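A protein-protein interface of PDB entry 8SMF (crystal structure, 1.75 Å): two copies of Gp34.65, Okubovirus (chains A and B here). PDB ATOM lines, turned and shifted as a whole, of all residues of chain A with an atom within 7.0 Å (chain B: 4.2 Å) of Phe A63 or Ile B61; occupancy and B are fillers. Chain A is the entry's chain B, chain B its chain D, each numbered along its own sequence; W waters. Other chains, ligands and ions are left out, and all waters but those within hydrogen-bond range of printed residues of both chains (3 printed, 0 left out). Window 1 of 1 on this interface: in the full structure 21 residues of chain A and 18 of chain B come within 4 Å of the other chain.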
ATOM      1  N   LEU A  15       6.987 -31.380  24.065  1.00  0.00           N
ATOM      2  CA  LEU A  15       7.369 -31.326  22.655  1.00  0.00           C
ATOM      3  C   LEU A  15       6.822 -32.520  21.885  1.00  0.00           C
ATOM      4  O   LEU A  15       6.305 -32.375  20.770  1.00  0.00           O
ATOM      5  CB  LEU A  15       8.892 -31.278  22.523  1.00  0.00           C
ATOM      6  CG  LEU A  15       9.603 -29.938  22.346  1.00  0.00           C
ATOM      7  CD1 LEU A  15      11.098 -30.172  22.215  1.00  0.00           C
ATOM      8  CD2 LEU A  15       9.076 -29.183  21.135  1.00  0.00           C
ATOM      9  N   VAL A  21       7.687 -25.130  23.361  1.00  0.00           N
ATOM     10  CA  VAL A  21       8.320 -24.888  24.650  1.00  0.00           C
ATOM     11  C   VAL A  21       9.427 -23.853  24.489  1.00  0.00           C
ATOM     12  O   VAL A  21       9.981 -23.662  23.406  1.00  0.00           O
ATOM     13  CB  VAL A  21       8.881 -26.183  25.282  1.00  0.00           C
ATOM     14  CG1 VAL A  21       7.759 -27.159  25.558  1.00  0.00           C
ATOM     15  CG2 VAL A  21       9.925 -26.822  24.377  1.00  0.00           C
ATOM     16  N   PHE A  32      10.769 -20.178  20.555  1.00  0.00           N
ATOM     17  CA  PHE A  32      10.216 -21.441  21.033  1.00  0.00           C
ATOM     18  C   PHE A  32      10.697 -22.582  20.150  1.00  0.00           C
ATOM     19  O   PHE A  32      11.134 -22.377  19.018  1.00  0.00           O
ATOM     20  CB  PHE A  32       8.679 -21.418  21.086  1.00  0.00           C
ATOM     21  CG  PHE A  32       8.015 -21.138  19.762  1.00  0.00           C
ATOM     22  CD1 PHE A  32       7.738 -22.167  18.871  1.00  0.00           C
ATOM     23  CD2 PHE A  32       7.654 -19.846  19.417  1.00  0.00           C
ATOM     24  CE1 PHE A  32       7.126 -21.908  17.658  1.00  0.00           C
ATOM     25  CE2 PHE A  32       7.034 -19.580  18.202  1.00  0.00           C
ATOM     26  CZ  PHE A  32       6.769 -20.609  17.325  1.00  0.00           C
ATOM     27  N   LEU A  33      10.622 -23.790  20.700  1.00  0.00           N
ATOM     28  CA  LEU A  33      10.921 -25.022  19.987  1.00  0.00           C
ATOM     29  C   LEU A  33       9.629 -25.667  19.504  1.00  0.00           C
ATOM     30  O   LEU A  33       8.576 -25.533  20.130  1.00  0.00           O
ATOM     31  CB  LEU A  33      11.664 -26.019  20.884  1.00  0.00           C
ATOM     32  CG  LEU A  33      12.898 -25.521  21.641  1.00  0.00           C
ATOM     33  CD1 LEU A  33      13.541 -26.656  22.427  1.00  0.00           C
ATOM     34  CD2 LEU A  33      13.886 -24.885  20.685  1.00  0.00           C
ATOM     35  N   PHE A  34       9.722 -26.376  18.385  1.00  0.00           N
ATOM     36  CA  PHE A  34       8.642 -27.248  17.953  1.00  0.00           C
ATOM     37  C   PHE A  34       9.253 -28.435  17.226  1.00  0.00           C
ATOM     38  O   PHE A  34      10.299 -28.316  16.588  1.00  0.00           O
ATOM     39  CB  PHE A  34       7.614 -26.509  17.079  1.00  0.00           C
ATOM     40  CG  PHE A  34       8.161 -25.958  15.787  1.00  0.00           C
ATOM     41  CD1 PHE A  34       8.835 -24.748  15.759  1.00  0.00           C
ATOM     42  CD2 PHE A  34       7.952 -26.628  14.589  1.00  0.00           C
ATOM     43  CE1 PHE A  34       9.314 -24.230  14.564  1.00  0.00           C
ATOM     44  CE2 PHE A  34       8.427 -26.118  13.398  1.00  0.00           C
ATOM     45  CZ  PHE A  34       9.105 -24.911  13.383  1.00  0.00           C
ATOM     46  N   LEU A  35       8.609 -29.588  17.362  1.00  0.00           N
ATOM     47  CA  LEU A  35       9.109 -30.851  16.835  1.00  0.00           C
ATOM     48  C   LEU A  35       8.272 -31.285  15.637  1.00  0.00           C
ATOM     49  O   LEU A  35       7.041 -31.295  15.709  1.00  0.00           O
ATOM     50  CB  LEU A  35       9.073 -31.930  17.923  1.00  0.00           C
ATOM     51  CG  LEU A  35       9.318 -33.389  17.516  1.00  0.00           C
ATOM     52  CD1 LEU A  35      10.754 -33.606  17.067  1.00  0.00           C
ATOM     53  CD2 LEU A  35       8.968 -34.312  18.678  1.00  0.00           C
ATOM     54  N   LYS A  36       8.939 -31.647  14.541  1.00  0.00           N
ATOM     55  CA  LYS A  36       8.285 -32.257  13.386  1.00  0.00           C
ATOM     56  C   LYS A  36       8.735 -33.707  13.258  1.00  0.00           C
ATOM     57  O   LYS A  36       9.935 -33.997  13.307  1.00  0.00           O
ATOM     58  CB  LYS A  36       8.602 -31.504  12.091  1.00  0.00           C
ATOM     59  CG  LYS A  36       8.330 -30.019  12.128  1.00  0.00           C
ATOM     60  CD  LYS A  36       6.917 -29.710  12.564  1.00  0.00           C
ATOM     61  CE  LYS A  36       5.901 -30.181  11.556  1.00  0.00           C
ATOM     62  NZ  LYS A  36       4.536 -29.648  11.885  1.00  0.00           N
ATOM     63  N   SER A  37       7.776 -34.609  13.077  1.00  0.00           N
ATOM     64  CA  SER A  37       8.089 -36.023  12.966  1.00  0.00           C
ATOM     65  C   SER A  37       8.526 -36.376  11.546  1.00  0.00           C
ATOM     66  O   SER A  37       8.378 -35.595  10.599  1.00  0.00           O
ATOM     67  CB  SER A  37       6.882 -36.871  13.361  1.00  0.00           C
ATOM     68  OG  SER A  37       5.868 -36.789  12.377  1.00  0.00           O
ATOM     69  N   LEU A  41       7.497 -34.388   8.156  1.00  0.00           N
ATOM     70  CA  LEU A  41       8.485 -33.781   7.272  1.00  0.00           C
ATOM     71  C   LEU A  41       8.379 -34.319   5.851  1.00  0.00           C
ATOM     72  O   LEU A  41       8.713 -33.612   4.894  1.00  0.00           O
ATOM     73  CB  LEU A  41       9.886 -34.013   7.837  1.00  0.00           C
ATOM     74  CG  LEU A  41      10.164 -33.253   9.137  1.00  0.00           C
ATOM     75  CD1 LEU A  41      11.359 -33.829   9.890  1.00  0.00           C
ATOM     76  CD2 LEU A  41      10.374 -31.775   8.843  1.00  0.00           C
ATOM     77  N   ASN A  60      13.287 -37.449  13.107  1.00  0.00           N
ATOM     78  CA  ASN A  60      12.638 -36.340  13.792  1.00  0.00           C
ATOM     79  C   ASN A  60      13.566 -35.133  13.782  1.00  0.00           C
ATOM     80  O   ASN A  60      14.776 -35.263  13.973  1.00  0.00           O
ATOM     81  CB  ASN A  60      12.290 -36.721  15.228  1.00  0.00           C
ATOM     82  CG  ASN A  60      11.354 -37.908  15.307  1.00  0.00           C
ATOM     83  OD1 ASN A  60      10.375 -37.989  14.570  1.00  0.00           O
ATOM     84  ND2 ASN A  60      11.661 -38.843  16.195  1.00  0.00           N
ATOM     85  N   ILE A  61      13.007 -33.955  13.537  1.00  0.00           N
ATOM     86  CA  ILE A  61      13.783 -32.722  13.590  1.00  0.00           C
ATOM     87  C   ILE A  61      13.098 -31.755  14.542  1.00  0.00           C
ATOM     88  O   ILE A  61      11.881 -31.554  14.460  1.00  0.00           O
ATOM     89  CB  ILE A  61      13.962 -32.086  12.199  1.00  0.00           C
ATOM     90  CG1 ILE A  61      14.749 -33.036  11.291  1.00  0.00           C
ATOM     91  CG2 ILE A  61      14.682 -30.748  12.319  1.00  0.00           C
ATOM     92  CD1 ILE A  61      14.937 -32.524   9.875  1.00  0.00           C
ATOM     93  N   ILE A  62      13.879 -31.175  15.452  1.00  0.00           N
ATOM     94  CA  ILE A  62      13.418 -30.112  16.334  1.00  0.00           C
ATOM     95  C   ILE A  62      13.844 -28.780  15.742  1.00  0.00           C
ATOM     96  O   ILE A  62      15.033 -28.567  15.465  1.00  0.00           O
ATOM     97  CB  ILE A  62      13.987 -30.272  17.752  1.00  0.00           C
ATOM     98  CG1 ILE A  62      13.712 -31.671  18.293  1.00  0.00           C
ATOM     99  CG2 ILE A  62      13.419 -29.187  18.672  1.00  0.00           C
ATOM    100  CD1 ILE A  62      14.436 -31.973  19.603  1.00  0.00           C
ATOM    101  N   PHE A  63      12.884 -27.883  15.552  1.00  0.00           N
ATOM    102  CA  PHE A  63      13.164 -26.540  15.075  1.00  0.00           C
ATOM    103  C   PHE A  63      13.001 -25.537  16.209  1.00  0.00           C
ATOM    104  O   PHE A  63      12.279 -25.769  17.182  1.00  0.00           O
ATOM    105  CB  PHE A  63      12.240 -26.148  13.917  1.00  0.00           C
ATOM    106  CG  PHE A  63      12.335 -27.053  12.719  1.00  0.00           C
ATOM    107  CD1 PHE A  63      11.545 -28.183  12.622  1.00  0.00           C
ATOM    108  CD2 PHE A  63      13.197 -26.756  11.679  1.00  0.00           C
ATOM    109  CE1 PHE A  63      11.627 -29.009  11.514  1.00  0.00           C
ATOM    110  CE2 PHE A  63      13.276 -27.571  10.569  1.00  0.00           C
ATOM    111  CZ  PHE A  63      12.494 -28.698  10.485  1.00  0.00           C
ATOM    112  N   ILE A  64      13.692 -24.410  16.069  1.00  0.00           N
ATOM    113  CA  ILE A  64      13.524 -23.265  16.953  1.00  0.00           C
ATOM    114  C   ILE A  64      13.085 -22.084  16.104  1.00  0.00           C
ATOM    115  O   ILE A  64      13.684 -21.806  15.058  1.00  0.00           O
ATOM    116  CB  ILE A  64      14.812 -22.941  17.731  1.00  0.00           C
ATOM    117  CG1 ILE A  64      14.635 -21.652  18.548  1.00  0.00           C
ATOM    118  CG2 ILE A  64      16.012 -22.841  16.798  1.00  0.00           C
ATOM    119  CD1 ILE A  64      15.782 -21.366  19.466  1.00  0.00           C
ATOM    120  N   LYS A  65      12.016 -21.420  16.530  1.00  0.00           N
ATOM    121  CA  LYS A  65      11.600 -20.159  15.937  1.00  0.00           C
ATOM    122  C   LYS A  65      12.365 -19.067  16.677  1.00  0.00           C
ATOM    123  O   LYS A  65      12.115 -18.816  17.857  1.00  0.00           O
ATOM    124  CB  LYS A  65      10.085 -19.996  16.050  1.00  0.00           C
ATOM    125  CG  LYS A  65       9.444 -19.036  15.049  1.00  0.00           C
ATOM    126  CD  LYS A  65       9.739 -17.578  15.372  1.00  0.00           C
ATOM    127  CE  LYS A  65       9.422 -17.248  16.827  1.00  0.00           C
ATOM    128  NZ  LYS A  65       9.805 -15.844  17.169  1.00  0.00           N
ATOM    129  N   ILE A  71      13.163 -19.748  11.098  1.00  0.00           N
ATOM    130  CA  ILE A  71      13.063 -21.126  11.560  1.00  0.00           C
ATOM    131  C   ILE A  71      14.409 -21.794  11.335  1.00  0.00           C
ATOM    132  O   ILE A  71      14.881 -21.887  10.195  1.00  0.00           O
ATOM    133  CB  ILE A  71      11.936 -21.882  10.841  1.00  0.00           C
ATOM    134  CG1 ILE A  71      10.599 -21.181  11.098  1.00  0.00           C
ATOM    135  CG2 ILE A  71      11.883 -23.328  11.306  1.00  0.00           C
ATOM    136  CD1 ILE A  71       9.478 -21.678  10.224  1.00  0.00           C
ATOM    137  N   HIS A  72      15.026 -22.248  12.424  1.00  0.00           N
ATOM    138  CA  HIS A  72      16.339 -22.871  12.411  1.00  0.00           C
ATOM    139  C   HIS A  72      16.256 -24.273  12.994  1.00  0.00           C
ATOM    140  O   HIS A  72      15.294 -24.627  13.678  1.00  0.00           O
ATOM    141  CB  HIS A  72      17.348 -22.056  13.226  1.00  0.00           C
ATOM    142  CG  HIS A  72      17.840 -20.828  12.529  1.00  0.00           C
ATOM    143  ND1 HIS A  72      18.902 -20.849  11.652  1.00  0.00           N
ATOM    144  CD2 HIS A  72      17.420 -19.543  12.584  1.00  0.00           C
ATOM    145  CE1 HIS A  72      19.114 -19.627  11.195  1.00  0.00           C
ATOM    146  NE2 HIS A  72      18.229 -18.817  11.745  1.00  0.00           N
ATOM    147  N   ALA A  73      17.285 -25.070  12.722  1.00  0.00           N
ATOM    148  CA  ALA A  73      17.460 -26.322  13.445  1.00  0.00           C
ATOM    149  C   ALA A  73      17.934 -26.028  14.861  1.00  0.00           C
ATOM    150  O   ALA A  73      18.868 -25.245  15.064  1.00  0.00           O
ATOM    151  CB  ALA A  73      18.464 -27.217  12.725  1.00  0.00           C
ATOM    152  N   TRP A  74      17.295 -26.649  15.849  1.00  0.00           N
ATOM    153  CA  TRP A  74      17.646 -26.412  17.244  1.00  0.00           C
ATOM    154  C   TRP A  74      18.784 -27.329  17.662  1.00  0.00           C
ATOM    155  O   TRP A  74      18.635 -28.555  17.667  1.00  0.00           O
ATOM    156  CB  TRP A  74      16.458 -26.625  18.174  1.00  0.00           C
ATOM    157  CG  TRP A  74      16.835 -26.385  19.609  1.00  0.00           C
ATOM    158  CD1 TRP A  74      17.329 -25.229  20.138  1.00  0.00           C
ATOM    159  CD2 TRP A  74      16.755 -27.318  20.693  1.00  0.00           C
ATOM    160  NE1 TRP A  74      17.558 -25.383  21.486  1.00  0.00           N
ATOM    161  CE2 TRP A  74      17.210 -26.654  21.852  1.00  0.00           C
ATOM    162  CE3 TRP A  74      16.337 -28.648  20.798  1.00  0.00           C
ATOM    163  CZ2 TRP A  74      17.268 -27.276  23.096  1.00  0.00           C
ATOM    164  CZ3 TRP A  74      16.390 -29.263  22.036  1.00  0.00           C
ATOM    165  CH2 TRP A  74      16.852 -28.577  23.169  1.00  0.00           C
ATOM    166  N   PHE B  34      25.391 -31.745   4.352  1.00  0.00           N
ATOM    167  CA  PHE B  34      25.096 -30.848   3.246  1.00  0.00           C
ATOM    168  C   PHE B  34      24.272 -29.676   3.752  1.00  0.00           C
ATOM    169  O   PHE B  34      23.453 -29.818   4.664  1.00  0.00           O
ATOM    170  CB  PHE B  34      24.382 -31.555   2.087  1.00  0.00           C
ATOM    171  CG  PHE B  34      23.058 -32.170   2.449  1.00  0.00           C
ATOM    172  CD1 PHE B  34      22.993 -33.434   3.019  1.00  0.00           C
ATOM    173  CD2 PHE B  34      21.875 -31.514   2.152  1.00  0.00           C
ATOM    174  CE1 PHE B  34      21.769 -34.013   3.322  1.00  0.00           C
ATOM    175  CE2 PHE B  34      20.651 -32.086   2.449  1.00  0.00           C
ATOM    176  CZ  PHE B  34      20.597 -33.338   3.032  1.00  0.00           C
ATOM    177  N   LEU B  35      24.501 -28.516   3.146  1.00  0.00           N
ATOM    178  CA  LEU B  35      23.875 -27.269   3.557  1.00  0.00           C
ATOM    179  C   LEU B  35      22.736 -26.915   2.612  1.00  0.00           C
ATOM    180  O   LEU B  35      22.873 -27.034   1.391  1.00  0.00           O
ATOM    181  CB  LEU B  35      24.901 -26.135   3.574  1.00  0.00           C
ATOM    182  CG  LEU B  35      24.354 -24.721   3.764  1.00  0.00           C
ATOM    183  CD1 LEU B  35      23.795 -24.550   5.169  1.00  0.00           C
ATOM    184  CD2 LEU B  35      25.419 -23.677   3.467  1.00  0.00           C
ATOM    185  N   LYS B  36      21.616 -26.475   3.183  1.00  0.00           N
ATOM    186  CA  LYS B  36      20.472 -25.985   2.423  1.00  0.00           C
ATOM    187  C   LYS B  36      20.191 -24.545   2.821  1.00  0.00           C
ATOM    188  O   LYS B  36      20.079 -24.239   4.010  1.00  0.00           O
ATOM    189  CB  LYS B  36      19.239 -26.859   2.669  1.00  0.00           C
ATOM    190  CG  LYS B  36      19.316 -28.210   1.974  1.00  0.00           C
ATOM    191  CD  LYS B  36      19.349 -27.998   0.472  1.00  0.00           C
ATOM    192  CE  LYS B  36      19.728 -29.254  -0.253  1.00  0.00           C
ATOM    193  NZ  LYS B  36      19.774 -29.011  -1.725  1.00  0.00           N
ATOM    194  N   LEU B  41      15.087 -24.222   1.238  1.00  0.00           N
ATOM    195  CA  LEU B  41      14.180 -24.797   2.228  1.00  0.00           C
ATOM    196  C   LEU B  41      12.761 -24.263   2.084  1.00  0.00           C
ATOM    197  O   LEU B  41      11.801 -24.989   2.363  1.00  0.00           O
ATOM    198  CB  LEU B  41      14.703 -24.524   3.639  1.00  0.00           C
ATOM    199  CG  LEU B  41      16.023 -25.224   3.964  1.00  0.00           C
ATOM    200  CD1 LEU B  41      16.605 -24.678   5.248  1.00  0.00           C
ATOM    201  CD2 LEU B  41      15.814 -26.727   4.053  1.00  0.00           C
ATOM    202  N   PHE B  47       5.550 -28.691   4.446  1.00  0.00           N
ATOM    203  CA  PHE B  47       4.705 -28.696   5.629  1.00  0.00           C
ATOM    204  C   PHE B  47       4.476 -27.266   6.106  1.00  0.00           C
ATOM    205  O   PHE B  47       5.425 -26.501   6.306  1.00  0.00           O
ATOM    206  CB  PHE B  47       5.323 -29.571   6.727  1.00  0.00           C
ATOM    207  CG  PHE B  47       6.554 -28.997   7.370  1.00  0.00           C
ATOM    208  CD1 PHE B  47       7.793 -29.107   6.761  1.00  0.00           C
ATOM    209  CD2 PHE B  47       6.477 -28.382   8.610  1.00  0.00           C
ATOM    210  CE1 PHE B  47       8.928 -28.593   7.367  1.00  0.00           C
ATOM    211  CE2 PHE B  47       7.607 -27.871   9.220  1.00  0.00           C
ATOM    212  CZ  PHE B  47       8.835 -27.973   8.596  1.00  0.00           C
ATOM    213  N   GLY B  59      16.002 -20.327   8.171  1.00  0.00           N
ATOM    214  CA  GLY B  59      17.418 -20.034   8.138  1.00  0.00           C
ATOM    215  C   GLY B  59      18.154 -21.091   7.333  1.00  0.00           C
ATOM    216  O   GLY B  59      17.563 -22.016   6.780  1.00  0.00           O
ATOM    217  N   ASN B  60      19.470 -20.938   7.249  1.00  0.00           N
ATOM    218  CA  ASN B  60      20.275 -21.999   6.658  1.00  0.00           C
ATOM    219  C   ASN B  60      20.313 -23.182   7.615  1.00  0.00           C
ATOM    220  O   ASN B  60      20.488 -23.010   8.822  1.00  0.00           O
ATOM    221  CB  ASN B  60      21.698 -21.522   6.373  1.00  0.00           C
ATOM    222  CG  ASN B  60      21.742 -20.271   5.523  1.00  0.00           C
ATOM    223  OD1 ASN B  60      21.406 -20.300   4.340  1.00  0.00           O
ATOM    224  ND2 ASN B  60      22.171 -19.163   6.122  1.00  0.00           N
ATOM    225  N   ILE B  61      20.143 -24.385   7.079  1.00  0.00           N
ATOM    226  CA  ILE B  61      20.137 -25.590   7.899  1.00  0.00           C
ATOM    227  C   ILE B  61      21.134 -26.578   7.311  1.00  0.00           C
ATOM    228  O   ILE B  61      21.105 -26.852   6.104  1.00  0.00           O
ATOM    229  CB  ILE B  61      18.732 -26.219   7.987  1.00  0.00           C
ATOM    230  CG1 ILE B  61      17.761 -25.245   8.666  1.00  0.00           C
ATOM    231  CG2 ILE B  61      18.791 -27.535   8.749  1.00  0.00           C
ATOM    232  CD1 ILE B  61      16.359 -25.792   8.872  1.00  0.00           C
ATOM    233  N   ILE B  62      22.010 -27.107   8.159  1.00  0.00           N
ATOM    234  CA  ILE B  62      22.931 -28.169   7.768  1.00  0.00           C
ATOM    235  C   ILE B  62      22.310 -29.506   8.134  1.00  0.00           C
ATOM    236  O   ILE B  62      21.866 -29.702   9.270  1.00  0.00           O
ATOM    237  CB  ILE B  62      24.296 -28.008   8.452  1.00  0.00           C
ATOM    238  CG1 ILE B  62      24.847 -26.595   8.256  1.00  0.00           C
ATOM    239  CG2 ILE B  62      25.282 -29.040   7.897  1.00  0.00           C
ATOM    240  CD1 ILE B  62      26.049 -26.308   9.149  1.00  0.00           C
ATOM    241  N   PHE B  63      22.285 -30.431   7.181  1.00  0.00           N
ATOM    242  CA  PHE B  63      21.756 -31.761   7.416  1.00  0.00           C
ATOM    243  C   PHE B  63      22.891 -32.772   7.433  1.00  0.00           C
ATOM    244  O   PHE B  63      23.939 -32.559   6.817  1.00  0.00           O
ATOM    245  CB  PHE B  63      20.736 -32.143   6.344  1.00  0.00           C
ATOM    246  CG  PHE B  63      19.527 -31.264   6.333  1.00  0.00           C
ATOM    247  CD1 PHE B  63      18.444 -31.555   7.149  1.00  0.00           C
ATOM    248  CD2 PHE B  63      19.475 -30.142   5.521  1.00  0.00           C
ATOM    249  CE1 PHE B  63      17.330 -30.750   7.153  1.00  0.00           C
ATOM    250  CE2 PHE B  63      18.360 -29.326   5.520  1.00  0.00           C
ATOM    251  CZ  PHE B  63      17.283 -29.633   6.338  1.00  0.00           C
HETATM  252  O   HOH W   1      19.801 -23.770  11.602  1.00  0.00           O
HETATM  253  O   HOH W   2      21.977 -21.148  10.264  1.00  0.00           O
HETATM  254  O   HOH W   3       7.705 -30.995   4.085  1.00  0.00           O
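Among the printed residues, merely in contact across the chains: Lys A36 with Phe B47 (3.5 Å), Leu A41 with Phe B47 (3.8 Å), Phe A63 with Ile B61 (3.9 Å), His A72 with Gly B59 (3.5 Å) and His A72 with Asn B60 (3.9 Å).
O of Phe A34 sits at hydrogen-bond distance from N of Phe A63 (2.8 Å).
The backbone carbonyl oxygen (O) of Ile A61 sits at hydrogen-bond distance from the backbone NH (N) of Lys A36 (2.9 Å).
N of Ile A64 is in hydrogen-bond range of O of His A72 (2.9 Å).
The backbone NH (N) of Lys B36 sits at hydrogen-bond distance from the backbone carbonyl oxygen (O) of Ile B61 (3.0 Å).
Hydrophobic or aromatic side chains of chain A that line the printed part of chain B: Leu A41, Phe A63 and His A72.
Of the 10 printed residues of chain B, 4 touch a printed residue of chain A.
Among the printed residues, no Asp or Glu carboxylate lies within 4 Å of a Lys or Arg side-chain nitrogen of the other chain.
Water W2 bridges the backbone carbonyl oxygen (O) of Asn B60 (2.8 Å) and a ring nitrogen (ND1) of His A72 (3.4 Å).
Water W3 bridges the backbone carbonyl oxygen of Leu A41 (2.9 Å) and the backbone NH of Phe B47 (3.2 Å).
Water W1 lies within hydrogen-bond range of the backbone carbonyl oxygen of Asn B60, the backbone NH of Ala A73 and a ring nitrogen (ND1) of His A72.
Of chain B, only Ile B61 comes within 4 Å of Phe A63.
Of the printed residues of chain A, Gly B59 touches Ile A71 (2.8 Å) and His A72 (3.5 Å).
Of the printed residues of chain A, Asn B60 touches His A72 (3.9 Å).
Printed residues of chain A within 4 Å of Ile B61: Phe A63 (3.9 Å).
The nearest printed residue of chain A that does not touch Ile B61 is Ala A73 (4.002 Å).
The nearest printed residue of chain A that does not touch Asn B60 is Ala A73 (5.5 Å).
Phe A63 touches Ile B61, but with the chains exchanged Ile A61 does not touch Phe B63 (4.04 Å).
Positions printed for both chains: 34, 35, 36, 41, 60, 61, 62 and 63.
Of the 6 pairs that touch across the chains among the printed residues, none has its exchanged pair printed and touching as well.
The backbone NH of Gly B59 sits at hydrogen-bond distance from the backbone carbonyl oxygen of Ile A71 (2.8 Å).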
